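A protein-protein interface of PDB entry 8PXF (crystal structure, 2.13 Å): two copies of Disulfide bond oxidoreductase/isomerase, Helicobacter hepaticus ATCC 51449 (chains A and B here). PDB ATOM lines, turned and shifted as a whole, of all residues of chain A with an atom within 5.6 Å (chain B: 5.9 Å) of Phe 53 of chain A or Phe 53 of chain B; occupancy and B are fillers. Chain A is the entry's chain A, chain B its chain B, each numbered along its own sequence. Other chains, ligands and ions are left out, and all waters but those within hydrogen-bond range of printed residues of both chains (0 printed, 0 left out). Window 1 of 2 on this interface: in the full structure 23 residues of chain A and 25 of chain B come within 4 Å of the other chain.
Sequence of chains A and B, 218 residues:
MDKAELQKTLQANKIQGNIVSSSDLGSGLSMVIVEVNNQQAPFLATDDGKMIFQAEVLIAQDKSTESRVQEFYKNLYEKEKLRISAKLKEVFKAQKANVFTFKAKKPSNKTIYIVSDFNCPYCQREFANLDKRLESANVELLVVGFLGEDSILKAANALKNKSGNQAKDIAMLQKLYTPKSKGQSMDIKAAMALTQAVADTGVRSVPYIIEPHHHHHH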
ATOM      1  N   LEU A  29     -19.964  -1.554 -23.766  1.00  0.00           N
ATOM      2  CA  LEU A  29     -20.454  -2.948 -23.950  1.00  0.00           C
ATOM      3  C   LEU A  29     -21.761  -3.147 -23.177  1.00  0.00           C
ATOM      4  O   LEU A  29     -21.956  -2.464 -22.157  1.00  0.00           O
ATOM      5  CB  LEU A  29     -19.394  -3.936 -23.453  1.00  0.00           C
ATOM      6  CG  LEU A  29     -18.118  -4.024 -24.286  1.00  0.00           C
ATOM      7  CD1 LEU A  29     -17.153  -5.027 -23.677  1.00  0.00           C
ATOM      8  CD2 LEU A  29     -18.435  -4.399 -25.723  1.00  0.00           C
ATOM      9  N   PRO A  42     -26.800 -16.009 -23.537  1.00  0.00           N
ATOM     10  CA  PRO A  42     -26.182 -14.736 -23.148  1.00  0.00           C
ATOM     11  C   PRO A  42     -24.939 -14.406 -23.964  1.00  0.00           C
ATOM     12  O   PRO A  42     -24.055 -15.245 -24.184  1.00  0.00           O
ATOM     13  CB  PRO A  42     -25.817 -14.990 -21.679  1.00  0.00           C
ATOM     14  CG  PRO A  42     -25.434 -16.463 -21.673  1.00  0.00           C
ATOM     15  CD  PRO A  42     -26.211 -17.142 -22.800  1.00  0.00           C
ATOM     16  N   PHE A  43     -24.860 -13.136 -24.375  1.00  0.00           N
ATOM     17  CA  PHE A  43     -23.797 -12.628 -25.230  1.00  0.00           C
ATOM     18  C   PHE A  43     -23.376 -11.255 -24.745  1.00  0.00           C
ATOM     19  O   PHE A  43     -24.068 -10.612 -23.951  1.00  0.00           O
ATOM     20  CB  PHE A  43     -24.243 -12.517 -26.681  1.00  0.00           C
ATOM     21  CG  PHE A  43     -24.348 -13.819 -27.368  1.00  0.00           C
ATOM     22  CD1 PHE A  43     -25.480 -14.618 -27.204  1.00  0.00           C
ATOM     23  CD2 PHE A  43     -23.322 -14.268 -28.165  1.00  0.00           C
ATOM     24  CE1 PHE A  43     -25.583 -15.859 -27.852  1.00  0.00           C
ATOM     25  CE2 PHE A  43     -23.410 -15.507 -28.804  1.00  0.00           C
ATOM     26  CZ  PHE A  43     -24.547 -16.301 -28.643  1.00  0.00           C
ATOM     27  N   LEU A  44     -22.240 -10.799 -25.263  1.00  0.00           N
ATOM     28  CA  LEU A  44     -21.765  -9.438 -25.051  1.00  0.00           C
ATOM     29  C   LEU A  44     -21.766  -8.711 -26.393  1.00  0.00           C
ATOM     30  O   LEU A  44     -21.546  -9.322 -27.442  1.00  0.00           O
ATOM     31  CB  LEU A  44     -20.357  -9.443 -24.441  1.00  0.00           C
ATOM     32  CG  LEU A  44     -20.143  -9.210 -22.941  1.00  0.00           C
ATOM     33  CD1 LEU A  44     -21.135  -9.957 -22.090  1.00  0.00           C
ATOM     34  CD2 LEU A  44     -18.752  -9.673 -22.572  1.00  0.00           C
ATOM     35  N   ALA A  45     -22.014  -7.403 -26.369  1.00  0.00           N
ATOM     36  CA  ALA A  45     -22.095  -6.670 -27.625  1.00  0.00           C
ATOM     37  C   ALA A  45     -21.646  -5.232 -27.431  1.00  0.00           C
ATOM     38  O   ALA A  45     -21.820  -4.647 -26.356  1.00  0.00           O
ATOM     39  CB  ALA A  45     -23.531  -6.672 -28.198  1.00  0.00           C
ATOM     40  N   THR A  46     -21.118  -4.657 -28.506  1.00  0.00           N
ATOM     41  CA  THR A  46     -20.776  -3.242 -28.528  1.00  0.00           C
ATOM     42  C   THR A  46     -22.046  -2.410 -28.676  1.00  0.00           C
ATOM     43  O   THR A  46     -23.013  -2.840 -29.310  1.00  0.00           O
ATOM     44  CB  THR A  46     -19.810  -2.941 -29.672  1.00  0.00           C
ATOM     45  OG1 THR A  46     -20.304  -3.558 -30.872  1.00  0.00           O
ATOM     46  CG2 THR A  46     -18.402  -3.478 -29.344  1.00  0.00           C
ATOM     47  N   MET A  51     -20.797  -5.579 -33.255  1.00  0.00           N
ATOM     48  CA  MET A  51     -19.998  -6.722 -32.843  1.00  0.00           C
ATOM     49  C   MET A  51     -20.649  -7.427 -31.661  1.00  0.00           C
ATOM     50  O   MET A  51     -21.072  -6.793 -30.695  1.00  0.00           O
ATOM     51  CB  MET A  51     -18.574  -6.266 -32.467  1.00  0.00           C
ATOM     52  CG  MET A  51     -17.612  -6.150 -33.643  1.00  0.00           C
ATOM     53  SD  MET A  51     -15.982  -5.520 -33.182  1.00  0.00           S
ATOM     54  CE  MET A  51     -15.815  -4.058 -34.193  1.00  0.00           C
ATOM     55  N   ILE A  52     -20.688  -8.746 -31.709  1.00  0.00           N
ATOM     56  CA  ILE A  52     -21.279  -9.520 -30.626  1.00  0.00           C
ATOM     57  C   ILE A  52     -20.397 -10.737 -30.383  1.00  0.00           C
ATOM     58  O   ILE A  52     -19.808 -11.282 -31.320  1.00  0.00           O
ATOM     59  CB  ILE A  52     -22.741  -9.885 -30.963  1.00  0.00           C
ATOM     60  CG1 ILE A  52     -23.459 -10.583 -29.803  1.00  0.00           C
ATOM     61  CG2 ILE A  52     -22.790 -10.723 -32.207  1.00  0.00           C
ATOM     62  CD1 ILE A  52     -24.970 -10.387 -29.860  1.00  0.00           C
ATOM     63  N   PHE A  53     -20.263 -11.140 -29.127  1.00  0.00           N
ATOM     64  CA  PHE A  53     -19.295 -12.181 -28.827  1.00  0.00           C
ATOM     65  C   PHE A  53     -19.620 -12.825 -27.491  1.00  0.00           C
ATOM     66  O   PHE A  53     -20.376 -12.286 -26.679  1.00  0.00           O
ATOM     67  CB  PHE A  53     -17.866 -11.610 -28.835  1.00  0.00           C
ATOM     68  CG  PHE A  53     -17.657 -10.475 -27.855  1.00  0.00           C
ATOM     69  CD1 PHE A  53     -17.953  -9.160 -28.212  1.00  0.00           C
ATOM     70  CD2 PHE A  53     -17.195 -10.726 -26.573  1.00  0.00           C
ATOM     71  CE1 PHE A  53     -17.765  -8.119 -27.305  1.00  0.00           C
ATOM     72  CE2 PHE A  53     -17.027  -9.696 -25.668  1.00  0.00           C
ATOM     73  CZ  PHE A  53     -17.303  -8.396 -26.034  1.00  0.00           C
ATOM     74  N   GLN A  54     -18.938 -13.931 -27.251  1.00  0.00           N
ATOM     75  CA  GLN A  54     -19.008 -14.649 -25.965  1.00  0.00           C
ATOM     76  C   GLN A  54     -17.584 -14.711 -25.424  1.00  0.00           C
ATOM     77  O   GLN A  54     -16.700 -15.108 -26.168  1.00  0.00           O
ATOM     78  CB  GLN A  54     -19.650 -16.011 -26.166  1.00  0.00           C
ATOM     79  CG  GLN A  54     -21.085 -16.057 -25.676  1.00  0.00           C
ATOM     80  CD  GLN A  54     -21.801 -17.328 -26.050  1.00  0.00           C
ATOM     81  OE1 GLN A  54     -21.369 -18.084 -26.909  1.00  0.00           O
ATOM     82  NE2 GLN A  54     -22.922 -17.563 -25.400  1.00  0.00           N
ATOM     83  N   ALA A  55     -17.388 -14.314 -24.174  1.00  0.00           N
ATOM     84  CA  ALA A  55     -16.057 -14.252 -23.575  1.00  0.00           C
ATOM     85  C   ALA A  55     -15.915 -15.361 -22.538  1.00  0.00           C
ATOM     86  O   ALA A  55     -16.601 -15.359 -21.510  1.00  0.00           O
ATOM     87  CB  ALA A  55     -15.794 -12.884 -22.952  1.00  0.00           C
ATOM     88  N   VAL A  57     -12.811 -15.951 -21.114  1.00  0.00           N
ATOM     89  CA  VAL A  57     -11.908 -15.260 -20.147  1.00  0.00           C
ATOM     90  C   VAL A  57     -12.273 -13.773 -20.131  1.00  0.00           C
ATOM     91  O   VAL A  57     -12.121 -13.114 -21.176  1.00  0.00           O
ATOM     92  CB  VAL A  57     -10.429 -15.468 -20.524  1.00  0.00           C
ATOM     93  CG1 VAL A  57     -10.077 -16.944 -20.617  1.00  0.00           C
ATOM     94  CG2 VAL A  57     -10.072 -14.757 -21.819  1.00  0.00           C
ATOM     95  N   LEU A  58     -12.775 -13.275 -18.997  1.00  0.00           N
ATOM     96  CA  LEU A  58     -13.135 -11.835 -18.881  1.00  0.00           C
ATOM     97  C   LEU A  58     -12.428 -11.217 -17.671  1.00  0.00           C
ATOM     98  O   LEU A  58     -12.588 -11.752 -16.559  1.00  0.00           O
ATOM     99  CB  LEU A  58     -14.653 -11.707 -18.735  1.00  0.00           C
ATOM    100  CG  LEU A  58     -15.158 -10.292 -18.464  1.00  0.00           C
ATOM    101  CD1 LEU A  58     -15.140  -9.460 -19.737  1.00  0.00           C
ATOM    102  CD2 LEU A  58     -16.555 -10.319 -17.870  1.00  0.00           C
ATOM    103  N   ILE A  59     -11.702 -10.117 -17.884  1.00  0.00           N
ATOM    104  CA  ILE A  59     -10.999  -9.402 -16.778  1.00  0.00           C
ATOM    105  C   ILE A  59     -11.499  -7.954 -16.770  1.00  0.00           C
ATOM    106  O   ILE A  59     -11.416  -7.302 -17.826  1.00  0.00           O
ATOM    107  CB  ILE A  59      -9.472  -9.487 -16.964  1.00  0.00           C
ATOM    108  CG1 ILE A  59      -9.053 -10.844 -17.537  1.00  0.00           C
ATOM    109  CG2 ILE A  59      -8.754  -9.177 -15.661  1.00  0.00           C
ATOM    110  CD1 ILE A  59      -7.587 -10.937 -17.888  1.00  0.00           C
ATOM    111  N   LEU B  29     -13.531  -1.093 -29.611  1.00  0.00           N
ATOM    112  CA  LEU B  29     -12.705  -2.259 -29.200  1.00  0.00           C
ATOM    113  C   LEU B  29     -11.322  -2.165 -29.851  1.00  0.00           C
ATOM    114  O   LEU B  29     -11.213  -1.548 -30.924  1.00  0.00           O
ATOM    115  CB  LEU B  29     -13.405  -3.560 -29.605  1.00  0.00           C
ATOM    116  CG  LEU B  29     -14.632  -3.943 -28.781  1.00  0.00           C
ATOM    117  CD1 LEU B  29     -15.217  -5.256 -29.271  1.00  0.00           C
ATOM    118  CD2 LEU B  29     -14.284  -4.040 -27.305  1.00  0.00           C
ATOM    119  N   PRO B  42      -2.447 -12.677 -27.319  1.00  0.00           N
ATOM    120  CA  PRO B  42      -3.403 -11.712 -27.884  1.00  0.00           C
ATOM    121  C   PRO B  42      -4.716 -11.609 -27.114  1.00  0.00           C
ATOM    122  O   PRO B  42      -5.297 -12.608 -26.681  1.00  0.00           O
ATOM    123  CB  PRO B  42      -3.646 -12.285 -29.284  1.00  0.00           C
ATOM    124  CG  PRO B  42      -3.580 -13.785 -29.070  1.00  0.00           C
ATOM    125  CD  PRO B  42      -2.576 -14.009 -27.951  1.00  0.00           C
ATOM    126  N   PHE B  43      -5.198 -10.377 -26.955  1.00  0.00           N
ATOM    127  CA  PHE B  43      -6.431 -10.121 -26.223  1.00  0.00           C
ATOM    128  C   PHE B  43      -7.247  -9.078 -26.955  1.00  0.00           C
ATOM    129  O   PHE B  43      -6.757  -8.369 -27.836  1.00  0.00           O
ATOM    130  CB  PHE B  43      -6.184  -9.622 -24.794  1.00  0.00           C
ATOM    131  CG  PHE B  43      -5.633 -10.665 -23.893  1.00  0.00           C
ATOM    132  CD1 PHE B  43      -4.283 -11.037 -23.978  1.00  0.00           C
ATOM    133  CD2 PHE B  43      -6.460 -11.329 -22.999  1.00  0.00           C
ATOM    134  CE1 PHE B  43      -3.765 -12.060 -23.167  1.00  0.00           C
ATOM    135  CE2 PHE B  43      -5.955 -12.341 -22.173  1.00  0.00           C
ATOM    136  CZ  PHE B  43      -4.607 -12.711 -22.260  1.00  0.00           C
ATOM    137  N   LEU B  44      -8.506  -8.986 -26.554  1.00  0.00           N
ATOM    138  CA  LEU B  44      -9.393  -7.922 -26.968  1.00  0.00           C
ATOM    139  C   LEU B  44      -9.698  -7.101 -25.724  1.00  0.00           C
ATOM    140  O   LEU B  44      -9.672  -7.621 -24.602  1.00  0.00           O
ATOM    141  CB  LEU B  44     -10.683  -8.475 -27.581  1.00  0.00           C
ATOM    142  CG  LEU B  44     -10.475  -9.207 -28.911  1.00  0.00           C
ATOM    143  CD1 LEU B  44     -11.807  -9.704 -29.490  1.00  0.00           C
ATOM    144  CD2 LEU B  44      -9.751  -8.276 -29.881  1.00  0.00           C
ATOM    145  N   ALA B  45      -9.915  -5.805 -25.914  1.00  0.00           N
ATOM    146  CA  ALA B  45     -10.181  -4.928 -24.785  1.00  0.00           C
ATOM    147  C   ALA B  45     -11.013  -3.743 -25.252  1.00  0.00           C
ATOM    148  O   ALA B  45     -11.010  -3.392 -26.435  1.00  0.00           O
ATOM    149  CB  ALA B  45      -8.897  -4.453 -24.133  1.00  0.00           C
ATOM    150  N   THR B  46     -11.731  -3.129 -24.314  1.00  0.00           N
ATOM    151  CA  THR B  46     -12.437  -1.894 -24.613  1.00  0.00           C
ATOM    152  C   THR B  46     -11.448  -0.738 -24.715  1.00  0.00           C
ATOM    153  O   THR B  46     -10.397  -0.737 -24.062  1.00  0.00           O
ATOM    154  CB  THR B  46     -13.474  -1.595 -23.540  1.00  0.00           C
ATOM    155  OG1 THR B  46     -12.848  -1.637 -22.244  1.00  0.00           O
ATOM    156  CG2 THR B  46     -14.611  -2.615 -23.634  1.00  0.00           C
ATOM    157  N   MET B  51     -11.732  -2.969 -19.634  1.00  0.00           N
ATOM    158  CA  MET B  51     -12.096  -4.408 -19.736  1.00  0.00           C
ATOM    159  C   MET B  51     -11.183  -5.140 -20.728  1.00  0.00           C
ATOM    160  O   MET B  51     -10.972  -4.616 -21.835  1.00  0.00           O
ATOM    161  CB  MET B  51     -13.561  -4.569 -20.153  1.00  0.00           C
ATOM    162  CG  MET B  51     -14.530  -4.152 -19.064  1.00  0.00           C
ATOM    163  SD  MET B  51     -16.261  -4.340 -19.540  1.00  0.00           S
ATOM    164  CE  MET B  51     -16.289  -3.383 -21.055  1.00  0.00           C
ATOM    165  N   ILE B  52     -10.695  -6.321 -20.336  1.00  0.00           N
ATOM    166  CA  ILE B  52      -9.833  -7.180 -21.202  1.00  0.00           C
ATOM    167  C   ILE B  52     -10.437  -8.589 -21.232  1.00  0.00           C
ATOM    168  O   ILE B  52     -10.754  -9.110 -20.151  1.00  0.00           O
ATOM    169  CB  ILE B  52      -8.375  -7.191 -20.708  1.00  0.00           C
ATOM    170  CG1 ILE B  52      -7.448  -7.859 -21.726  1.00  0.00           C
ATOM    171  CG2 ILE B  52      -8.278  -7.846 -19.340  1.00  0.00           C
ATOM    172  CD1 ILE B  52      -5.984  -7.569 -21.505  1.00  0.00           C
ATOM    173  N   PHE B  53     -10.566  -9.182 -22.422  1.00  0.00           N
ATOM    174  CA  PHE B  53     -11.178 -10.530 -22.555  1.00  0.00           C
ATOM    175  C   PHE B  53     -10.708 -11.193 -23.853  1.00  0.00           C
ATOM    176  O   PHE B  53     -10.111 -10.503 -24.695  1.00  0.00           O
ATOM    177  CB  PHE B  53     -12.700 -10.398 -22.603  1.00  0.00           C
ATOM    178  CG  PHE B  53     -13.188  -9.484 -23.698  1.00  0.00           C
ATOM    179  CD1 PHE B  53     -13.355  -8.128 -23.469  1.00  0.00           C
ATOM    180  CD2 PHE B  53     -13.453  -9.973 -24.966  1.00  0.00           C
ATOM    181  CE1 PHE B  53     -13.792  -7.286 -24.478  1.00  0.00           C
ATOM    182  CE2 PHE B  53     -13.891  -9.130 -25.973  1.00  0.00           C
ATOM    183  CZ  PHE B  53     -14.060  -7.788 -25.728  1.00  0.00           C
ATOM    184  N   GLN B  54     -10.936 -12.504 -23.984  1.00  0.00           N
ATOM    185  CA  GLN B  54     -10.579 -13.212 -25.230  1.00  0.00           C
ATOM    186  C   GLN B  54     -11.871 -13.825 -25.723  1.00  0.00           C
ATOM    187  O   GLN B  54     -12.616 -14.305 -24.905  1.00  0.00           O
ATOM    188  CB  GLN B  54      -9.562 -14.329 -25.057  1.00  0.00           C
ATOM    189  CG  GLN B  54      -8.234 -13.864 -24.500  1.00  0.00           C
ATOM    190  CD  GLN B  54      -7.104 -14.781 -24.879  1.00  0.00           C
ATOM    191  OE1 GLN B  54      -6.916 -15.119 -26.034  1.00  0.00           O
ATOM    192  NE2 GLN B  54      -6.334 -15.191 -23.896  1.00  0.00           N
ATOM    193  N   ALA B  55     -12.156 -13.823 -27.010  1.00  0.00           N
ATOM    194  CA  ALA B  55     -13.488 -14.351 -27.344  1.00  0.00           C
ATOM    195  C   ALA B  55     -13.410 -15.675 -28.085  1.00  0.00           C
ATOM    196  O   ALA B  55     -12.784 -15.708 -29.139  1.00  0.00           O
ATOM    197  CB  ALA B  55     -14.221 -13.335 -28.159  1.00  0.00           C
ATOM    198  N   VAL B  57     -16.132 -17.194 -29.311  1.00  0.00           N
ATOM    199  CA  VAL B  57     -17.087 -16.918 -30.425  1.00  0.00           C
ATOM    200  C   VAL B  57     -17.202 -15.405 -30.616  1.00  0.00           C
ATOM    201  O   VAL B  57     -17.610 -14.718 -29.662  1.00  0.00           O
ATOM    202  CB  VAL B  57     -18.467 -17.532 -30.122  1.00  0.00           C
ATOM    203  CG1 VAL B  57     -19.503 -17.136 -31.162  1.00  0.00           C
ATOM    204  CG2 VAL B  57     -18.397 -19.043 -29.973  1.00  0.00           C
ATOM    205  N   LEU B  58     -16.857 -14.915 -31.809  1.00  0.00           N
ATOM    206  CA  LEU B  58     -16.980 -13.468 -32.119  1.00  0.00           C
ATOM    207  C   LEU B  58     -17.792 -13.305 -33.406  1.00  0.00           C
ATOM    208  O   LEU B  58     -17.409 -13.909 -34.425  1.00  0.00           O
ATOM    209  CB  LEU B  58     -15.586 -12.852 -32.271  1.00  0.00           C
ATOM    210  CG  LEU B  58     -15.566 -11.471 -32.922  1.00  0.00           C
ATOM    211  CD1 LEU B  58     -14.281 -10.729 -32.599  1.00  0.00           C
ATOM    212  CD2 LEU B  58     -15.757 -11.579 -34.426  1.00  0.00           C
ATOM    213  N   ILE B  59     -18.855 -12.500 -33.355  1.00  0.00           N
ATOM    214  CA  ILE B  59     -19.709 -12.243 -34.551  1.00  0.00           C
ATOM    215  C   ILE B  59     -19.604 -10.748 -34.862  1.00  0.00           C
ATOM    216  O   ILE B  59     -19.900  -9.943 -33.962  1.00  0.00           O
ATOM    217  CB  ILE B  59     -21.159 -12.679 -34.270  1.00  0.00           C
ATOM    218  CG1 ILE B  59     -21.214 -14.100 -33.703  1.00  0.00           C
ATOM    219  CG2 ILE B  59     -22.018 -12.535 -35.516  1.00  0.00           C
ATOM    220  CD1 ILE B  59     -22.508 -14.438 -33.005  1.00  0.00           C
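Leu 29 of chain A touches Thr 46 of chain B, and with the chains exchanged Thr 46 of chain A touches Leu 29 of chain B. Ile 52 of chain A touches Leu 58 of chain B, and with the chains exchanged Leu 58 of chain A touches Ile 52 of chain B. Phe 53 of chain A touches Leu 58 of chain B, and with the chains exchanged Leu 58 of chain A touches Phe 53 of chain B. Gln 54 of chain A touches Ala 55 of chain B, and with the chains exchanged Ala 55 of chain A touches Gln 54 of chain B. Of the 20 pairs that touch across the chains among the printed residues, 19 have their exchanged pair printed and touching as well.
Along chain B the printed residues that touch a printed residue of chain A span positions 29 to 59. Among the printed residues, 20 pairs touch across the chains. Among the printed residues, no Asp or Glu carboxylate lies within 4 Å of a Lys or Arg side-chain nitrogen of the other chain.
The backbone NH (N) of Ile 59 of chain B sits at hydrogen-bond distance from the backbone carbonyl oxygen (O) of Ile 52 of chain A (2.6 Å). O of Val 57 of chain B lies within hydrogen-bond range of N of Gln 54 of chain A, 2.9 Å away. The backbone NH (N) of Gln 54 of chain B lies within hydrogen-bond range of the backbone carbonyl oxygen (O) of Val 57 of chain A, 3.1 Å away. The backbone carbonyl oxygen (O) of Ile 52 of chain B is in hydrogen-bond range of the backbone NH (N) of Ile 59 of chain A.
Among the printed residues, merely in contact across the chains: Leu 29 of chain A with Thr 46 of chain B, Leu 29 of chain A with Met 51 of chain B, Thr 46 of chain A with Leu 29 of chain B, Met 51 of chain A with Leu 29 of chain B, Met 51 of chain A with Ile 59 of chain B, Ile 52 of chain A with Leu 58 of chain B, Phe 53 of chain A with Phe 53 of chain B, Phe 53 of chain A with Val 57 of chain B, Phe 53 of chain A with Leu 58 of chain B, Gln 54 of chain A with Ala 55 of chain B, Ala 55 of chain A with Phe 53 of chain B, Ala 55 of chain A with Gln 54 of chain B, Val 57 of chain A with Phe 53 of chain B, Leu 58 of chain A with Ile 52 of chain B, Leu 58 of chain A with Phe 53 of chain B and Ile 59 of chain A with Met 51 of chain B.
Of the printed residues of chain A, Phe 53 of chain B touches Phe 53 (3.2 Å), Ala 55 (3.98 Å), Val 57 (3.1 Å) and Leu 58 (3.9 Å). Of the printed residues of chain A, Ile 59 of chain B touches Met 51 and Ile 52. Of the printed residues of chain B, Val 57 of chain A touches Phe 53 and Gln 54. Ala 45 of chain A touches none of the printed residues of chain B. Pro 42 of chain B touches none of the printed residues of chain A. The nearest residue of chain B that does not touch Phe 53 of chain A is Ala 55 of chain B (4.1 Å).
O of Pro 42 of chain A sits at hydrogen-bond distance from NE2 of Gln 54 of chain A, 2.9 Å away. N of Leu 44 of chain A sits at hydrogen-bond distance from O of Phe 53 of chain A, 2.8 Å away. The backbone NH (N) of Thr 46 of chain A lies within hydrogen-bond range of the backbone carbonyl oxygen (O) of Met 51 of chain A, 3.1 Å away. The side-chain amide oxygen (OE1) of Gln 54 of chain B sits close to the backbone carbonyl oxygen (O) of Pro 42 of chain B (3.1 Å). The backbone carbonyl oxygen of Leu 44 of chain B lies within hydrogen-bond range of the backbone NH of Phe 53 of chain B (2.8 Å). The backbone NH (N) of Thr 46 of chain B sits at hydrogen-bond distance from the backbone carbonyl oxygen (O) of Met 51 of chain B.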
